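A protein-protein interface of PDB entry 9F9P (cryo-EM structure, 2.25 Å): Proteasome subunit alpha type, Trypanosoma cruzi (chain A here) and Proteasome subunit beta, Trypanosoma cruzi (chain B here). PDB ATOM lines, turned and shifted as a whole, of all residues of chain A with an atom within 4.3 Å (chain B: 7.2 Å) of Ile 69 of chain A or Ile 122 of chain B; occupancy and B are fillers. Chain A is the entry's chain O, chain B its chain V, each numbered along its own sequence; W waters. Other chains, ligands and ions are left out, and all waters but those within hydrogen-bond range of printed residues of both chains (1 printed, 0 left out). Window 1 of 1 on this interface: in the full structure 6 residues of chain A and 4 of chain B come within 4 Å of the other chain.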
ATOM      1  N   HIS A  67     -12.580  18.150   8.042  1.00  0.00           N
ATOM      2  CA  HIS A  67     -11.708  17.041   7.723  1.00  0.00           C
ATOM      3  C   HIS A  67     -10.899  16.671   8.957  1.00  0.00           C
ATOM      4  O   HIS A  67     -10.639  17.526   9.788  1.00  0.00           O
ATOM      5  CB  HIS A  67     -10.679  17.414   6.651  1.00  0.00           C
ATOM      6  CG  HIS A  67     -11.269  17.953   5.382  1.00  0.00           C
ATOM      7  ND1 HIS A  67     -11.641  17.084   4.377  1.00  0.00           N
ATOM      8  CD2 HIS A  67     -11.679  19.204   5.001  1.00  0.00           C
ATOM      9  CE1 HIS A  67     -12.207  17.800   3.415  1.00  0.00           C
ATOM     10  NE2 HIS A  67     -12.228  19.091   3.758  1.00  0.00           N
ATOM     11  N   ASN A  68     -10.512  15.405   9.071  1.00  0.00           N
ATOM     12  CA  ASN A  68      -9.591  14.961  10.101  1.00  0.00           C
ATOM     13  C   ASN A  68      -8.164  15.130   9.581  1.00  0.00           C
ATOM     14  O   ASN A  68      -7.883  14.789   8.428  1.00  0.00           O
ATOM     15  CB  ASN A  68      -9.775  13.487  10.452  1.00  0.00           C
ATOM     16  CG  ASN A  68     -10.998  13.220  11.274  1.00  0.00           C
ATOM     17  OD1 ASN A  68     -12.107  13.153  10.741  1.00  0.00           O
ATOM     18  ND2 ASN A  68     -10.803  13.015  12.568  1.00  0.00           N
ATOM     19  N   ILE A  69      -7.305  15.668  10.435  1.00  0.00           N
ATOM     20  CA  ILE A  69      -5.885  15.726  10.203  1.00  0.00           C
ATOM     21  C   ILE A  69      -5.261  14.444  10.725  1.00  0.00           C
ATOM     22  O   ILE A  69      -4.334  13.907  10.137  1.00  0.00           O
ATOM     23  CB  ILE A  69      -5.252  16.937  10.911  1.00  0.00           C
ATOM     24  CG1 ILE A  69      -5.860  18.276  10.509  1.00  0.00           C
ATOM     25  CG2 ILE A  69      -3.762  16.959  10.698  1.00  0.00           C
ATOM     26  CD1 ILE A  69      -5.963  18.469   9.030  1.00  0.00           C
ATOM     27  N   ASN A  70      -5.648  14.057  11.932  1.00  0.00           N
ATOM     28  CA  ASN A  70      -5.435  12.693  12.381  1.00  0.00           C
ATOM     29  C   ASN A  70      -6.682  12.307  13.147  1.00  0.00           C
ATOM     30  O   ASN A  70      -7.699  12.986  13.024  1.00  0.00           O
ATOM     31  CB  ASN A  70      -4.107  12.586  13.118  1.00  0.00           C
ATOM     32  CG  ASN A  70      -4.074  13.345  14.429  1.00  0.00           C
ATOM     33  OD1 ASN A  70      -5.093  13.643  15.046  1.00  0.00           O
ATOM     34  ND2 ASN A  70      -2.863  13.621  14.886  1.00  0.00           N
ATOM     35  N   ILE A  73      -7.554  15.386  15.819  1.00  0.00           N
ATOM     36  CA  ILE A  73      -7.552  16.787  15.442  1.00  0.00           C
ATOM     37  C   ILE A  73      -8.435  16.948  14.212  1.00  0.00           C
ATOM     38  O   ILE A  73      -8.241  16.263  13.238  1.00  0.00           O
ATOM     39  CB  ILE A  73      -6.126  17.266  15.102  1.00  0.00           C
ATOM     40  CG1 ILE A  73      -5.202  17.172  16.304  1.00  0.00           C
ATOM     41  CG2 ILE A  73      -6.136  18.685  14.563  1.00  0.00           C
ATOM     42  CD1 ILE A  73      -3.792  17.578  16.020  1.00  0.00           C
ATOM     43  N   THR A  75     -10.155  19.926  11.388  1.00  0.00           N
ATOM     44  CA  THR A  75     -10.164  21.247  10.789  1.00  0.00           C
ATOM     45  C   THR A  75     -11.501  21.606  10.161  1.00  0.00           C
ATOM     46  O   THR A  75     -12.174  20.751   9.636  1.00  0.00           O
ATOM     47  CB  THR A  75      -9.313  21.440   9.523  1.00  0.00           C
ATOM     48  OG1 THR A  75      -8.871  20.285   8.803  1.00  0.00           O
ATOM     49  CG2 THR A  75      -8.095  22.244   9.841  1.00  0.00           C
ATOM     50  N   ALA A  91      -0.827  19.771   6.220  1.00  0.00           N
ATOM     51  CA  ALA A  91      -1.009  19.476   7.629  1.00  0.00           C
ATOM     52  C   ALA A  91      -0.956  17.971   7.960  1.00  0.00           C
ATOM     53  O   ALA A  91      -0.478  17.591   9.020  1.00  0.00           O
ATOM     54  CB  ALA A  91      -2.348  20.044   8.064  1.00  0.00           C
ATOM     55  N   ARG A  92      -1.530  17.117   7.101  1.00  0.00           N
ATOM     56  CA  ARG A  92      -1.549  15.674   7.311  1.00  0.00           C
ATOM     57  C   ARG A  92      -0.116  15.168   7.265  1.00  0.00           C
ATOM     58  O   ARG A  92       0.276  14.359   8.112  1.00  0.00           O
ATOM     59  CB  ARG A  92      -2.439  14.988   6.273  1.00  0.00           C
ATOM     60  CG  ARG A  92      -3.908  14.970   6.669  1.00  0.00           C
ATOM     61  CD  ARG A  92      -4.820  14.463   5.559  1.00  0.00           C
ATOM     62  NE  ARG A  92      -6.204  14.450   6.017  1.00  0.00           N
ATOM     63  CZ  ARG A  92      -7.232  14.159   5.247  1.00  0.00           C
ATOM     64  NH1 ARG A  92      -7.049  13.823   4.010  1.00  0.00           N
ATOM     65  NH2 ARG A  92      -8.459  14.214   5.687  1.00  0.00           N
ATOM     66  N   ALA A  95       1.766  16.211  10.436  1.00  0.00           N
ATOM     67  CA  ALA A  95       1.447  15.458  11.639  1.00  0.00           C
ATOM     68  C   ALA A  95       2.090  14.070  11.623  1.00  0.00           C
ATOM     69  O   ALA A  95       2.396  13.513  12.685  1.00  0.00           O
ATOM     70  CB  ALA A  95      -0.032  15.352  11.792  1.00  0.00           C
ATOM     71  N   LEU A 111       0.788  21.930  15.880  1.00  0.00           N
ATOM     72  CA  LEU A 111       0.400  21.809  14.483  1.00  0.00           C
ATOM     73  C   LEU A 111      -0.043  23.145  13.906  1.00  0.00           C
ATOM     74  O   LEU A 111       0.312  23.463  12.783  1.00  0.00           O
ATOM     75  CB  LEU A 111      -0.758  20.818  14.367  1.00  0.00           C
ATOM     76  CG  LEU A 111      -1.335  20.706  12.951  1.00  0.00           C
ATOM     77  CD1 LEU A 111      -0.509  19.810  12.057  1.00  0.00           C
ATOM     78  CD2 LEU A 111      -2.736  20.219  13.013  1.00  0.00           C
ATOM     79  N   LEU B 117       0.187   3.001   7.253  1.00  0.00           N
ATOM     80  CA  LEU B 117      -1.193   2.536   7.354  1.00  0.00           C
ATOM     81  C   LEU B 117      -2.097   3.567   7.997  1.00  0.00           C
ATOM     82  O   LEU B 117      -3.279   3.591   7.704  1.00  0.00           O
ATOM     83  CB  LEU B 117      -1.313   1.220   8.146  1.00  0.00           C
ATOM     84  CG  LEU B 117      -0.784  -0.048   7.457  1.00  0.00           C
ATOM     85  CD1 LEU B 117      -0.693  -1.217   8.437  1.00  0.00           C
ATOM     86  CD2 LEU B 117      -1.649  -0.440   6.276  1.00  0.00           C
ATOM     87  N   GLU B 118      -1.560   4.327   8.952  1.00  0.00           N
ATOM     88  CA  GLU B 118      -2.295   5.377   9.661  1.00  0.00           C
ATOM     89  C   GLU B 118      -2.640   6.517   8.692  1.00  0.00           C
ATOM     90  O   GLU B 118      -3.771   6.958   8.663  1.00  0.00           O
ATOM     91  CB  GLU B 118      -1.414   5.843  10.828  1.00  0.00           C
ATOM     92  CG  GLU B 118      -2.118   6.668  11.885  1.00  0.00           C
ATOM     93  CD  GLU B 118      -1.255   7.273  12.993  1.00  0.00           C
ATOM     94  OE1 GLU B 118       0.010   7.179  12.910  1.00  0.00           O
ATOM     95  OE2 GLU B 118      -1.847   7.841  13.964  1.00  0.00           O
ATOM     96  N   SER B 119      -1.658   6.990   7.916  1.00  0.00           N
ATOM     97  CA  SER B 119      -1.882   7.933   6.822  1.00  0.00           C
ATOM     98  C   SER B 119      -2.917   7.471   5.798  1.00  0.00           C
ATOM     99  O   SER B 119      -3.651   8.284   5.281  1.00  0.00           O
ATOM    100  CB  SER B 119      -0.603   8.227   6.053  1.00  0.00           C
ATOM    101  OG  SER B 119       0.358   8.835   6.897  1.00  0.00           O
ATOM    102  N   TYR B 120      -2.874   6.195   5.392  1.00  0.00           N
ATOM    103  CA  TYR B 120      -3.764   5.666   4.377  1.00  0.00           C
ATOM    104  C   TYR B 120      -5.184   5.681   4.902  1.00  0.00           C
ATOM    105  O   TYR B 120      -6.116   5.982   4.184  1.00  0.00           O
ATOM    106  CB  TYR B 120      -3.367   4.226   4.014  1.00  0.00           C
ATOM    107  CG  TYR B 120      -4.191   3.630   2.897  1.00  0.00           C
ATOM    108  CD1 TYR B 120      -4.096   4.141   1.614  1.00  0.00           C
ATOM    109  CD2 TYR B 120      -5.144   2.643   3.132  1.00  0.00           C
ATOM    110  CE1 TYR B 120      -4.908   3.686   0.593  1.00  0.00           C
ATOM    111  CE2 TYR B 120      -5.917   2.129   2.100  1.00  0.00           C
ATOM    112  CZ  TYR B 120      -5.816   2.665   0.835  1.00  0.00           C
ATOM    113  OH  TYR B 120      -6.604   2.239  -0.200  1.00  0.00           O
ATOM    114  N   GLU B 121      -5.342   5.307   6.161  1.00  0.00           N
ATOM    115  CA  GLU B 121      -6.637   5.232   6.802  1.00  0.00           C
ATOM    116  C   GLU B 121      -7.286   6.611   6.935  1.00  0.00           C
ATOM    117  O   GLU B 121      -8.508   6.721   6.880  1.00  0.00           O
ATOM    118  CB  GLU B 121      -6.460   4.544   8.154  1.00  0.00           C
ATOM    119  CG  GLU B 121      -7.750   4.421   8.931  1.00  0.00           C
ATOM    120  CD  GLU B 121      -7.706   3.706  10.279  1.00  0.00           C
ATOM    121  OE1 GLU B 121      -6.563   3.383  10.769  1.00  0.00           O
ATOM    122  OE2 GLU B 121      -8.832   3.470  10.854  1.00  0.00           O
ATOM    123  N   ILE B 122      -6.478   7.671   7.094  1.00  0.00           N
ATOM    124  CA  ILE B 122      -7.013   9.020   7.222  1.00  0.00           C
ATOM    125  C   ILE B 122      -7.470   9.539   5.866  1.00  0.00           C
ATOM    126  O   ILE B 122      -8.534  10.112   5.774  1.00  0.00           O
ATOM    127  CB  ILE B 122      -5.996   9.945   7.922  1.00  0.00           C
ATOM    128  CG1 ILE B 122      -5.983   9.760   9.436  1.00  0.00           C
ATOM    129  CG2 ILE B 122      -6.243  11.406   7.621  1.00  0.00           C
ATOM    130  CD1 ILE B 122      -4.580  10.045  10.043  1.00  0.00           C
ATOM    131  N   ASP B 123      -6.674   9.296   4.830  1.00  0.00           N
ATOM    132  CA  ASP B 123      -6.956   9.654   3.442  1.00  0.00           C
ATOM    133  C   ASP B 123      -8.207   8.977   2.840  1.00  0.00           C
ATOM    134  O   ASP B 123      -8.892   9.591   2.044  1.00  0.00           O
ATOM    135  CB  ASP B 123      -5.709   9.333   2.629  1.00  0.00           C
ATOM    136  CG  ASP B 123      -5.659   9.919   1.227  1.00  0.00           C
ATOM    137  OD1 ASP B 123      -6.400  10.911   0.960  1.00  0.00           O
ATOM    138  OD2 ASP B 123      -4.878   9.375   0.393  1.00  0.00           O
ATOM    139  N   THR B 124      -8.568   7.754   3.230  1.00  0.00           N
ATOM    140  CA  THR B 124      -9.745   7.069   2.702  1.00  0.00           C
ATOM    141  C   THR B 124     -10.937   7.122   3.672  1.00  0.00           C
ATOM    142  O   THR B 124     -12.058   6.780   3.293  1.00  0.00           O
ATOM    143  CB  THR B 124      -9.440   5.581   2.387  1.00  0.00           C
ATOM    144  OG1 THR B 124      -9.210   4.780   3.552  1.00  0.00           O
ATOM    145  CG2 THR B 124      -8.193   5.405   1.549  1.00  0.00           C
ATOM    146  N   SER B 125     -10.700   7.429   4.943  1.00  0.00           N
ATOM    147  CA  SER B 125     -11.760   7.453   5.945  1.00  0.00           C
ATOM    148  C   SER B 125     -12.377   6.071   6.212  1.00  0.00           C
ATOM    149  O   SER B 125     -13.494   5.980   6.705  1.00  0.00           O
ATOM    150  CB  SER B 125     -12.834   8.483   5.593  1.00  0.00           C
ATOM    151  OG  SER B 125     -12.314   9.807   5.517  1.00  0.00           O
ATOM    152  N   LYS B 126     -11.628   4.989   5.977  1.00  0.00           N
ATOM    153  CA  LYS B 126     -12.104   3.629   6.209  1.00  0.00           C
ATOM    154  C   LYS B 126     -11.019   2.803   6.893  1.00  0.00           C
ATOM    155  O   LYS B 126      -9.845   3.134   6.828  1.00  0.00           O
ATOM    156  CB  LYS B 126     -12.433   2.941   4.885  1.00  0.00           C
ATOM    157  CG  LYS B 126     -13.784   3.300   4.289  1.00  0.00           C
ATOM    158  CD  LYS B 126     -14.122   2.418   3.112  1.00  0.00           C
ATOM    159  CE  LYS B 126     -14.421   0.984   3.513  1.00  0.00           C
ATOM    160  NZ  LYS B 126     -14.435   0.073   2.344  1.00  0.00           N
ATOM    161  N   VAL B 128      -8.390  -0.322   7.283  1.00  0.00           N
ATOM    162  CA  VAL B 128      -7.580  -0.966   6.261  1.00  0.00           C
ATOM    163  C   VAL B 128      -7.741  -2.486   6.306  1.00  0.00           C
ATOM    164  O   VAL B 128      -7.970  -3.078   7.356  1.00  0.00           O
ATOM    165  CB  VAL B 128      -6.098  -0.581   6.406  1.00  0.00           C
ATOM    166  CG1 VAL B 128      -5.901   0.907   6.389  1.00  0.00           C
ATOM    167  CG2 VAL B 128      -5.495  -1.090   7.679  1.00  0.00           C
HETATM  168  O   HOH W   1      -4.322  12.392   2.814  1.00  0.00           O
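ND2 of Asn 68 of chain A lies within hydrogen-bond range of O of Asn 70 of chain A (3.1 Å). The backbone carbonyl oxygen of Asn 68 of chain A sits at hydrogen-bond distance from the guanidinium group of Arg 92 of chain A (2.9 Å). OD1 of Asn 70 of chain A is in hydrogen-bond range of N of Ile 73 of chain A, 3.1 Å away.
O of Asn 68 of chain A touches CG2 of Ile 122 of chain B, at 3.8 Å. O of Ile 69 of chain A touches CD1 of Ile 122 of chain B, at 3.9 Å. Asn 70 of chain A touches Ile 122 of chain B (CA to CD1, 3.6 Å). NE of Arg 92 of chain A touches CG2 of Ile 122 of chain B, 3.4 Å away.
Printed residues of chain B within 4 Å of Asn 68 of chain A: Ile 122. Ile 69 of chain A touches just one residue of chain B: Ile 122 (3.9 Å). Of the printed residues of chain B, Asn 70 of chain A touches Ile 122. Of the printed residues of chain B, Arg 92 of chain A touches Ile 122 (3.4 Å). Ile 122 of chain B touches just these residues of chain A: Asn 68 (3.8 Å), Ile 69 (3.9 Å), Asn 70 (3.6 Å) and Arg 92 (3.4 Å). The nearest residue of chain B that does not touch Ile 69 of chain A is Glu 118 of chain B (7.1 Å). The nearest printed residue of chain A that does not touch Ile 122 of chain B is His 67 of chain A (7.2 Å).
Of the 11 printed residues of chain B, 1 touches a printed residue of chain A. Printed residues of chain B that touch a printed residue of chain A: Ile 122. Hydrophobic or aromatic side chains of chain B within 4 Å of the printed part of chain A: Ile 122. Printed residues of chain A that touch a printed residue of chain B: Asn 68, Ile 69, Asn 70 and Arg 92. Among the printed residues, no Asp or Glu carboxylate lies within 4 Å of a Lys or Arg side-chain nitrogen of the other chain.
Water W1 lies within hydrogen-bond range of OD1 of Asp 123 of chain B (3.2 Å) and NH1 of Arg 92 of chain A (3.3 Å).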
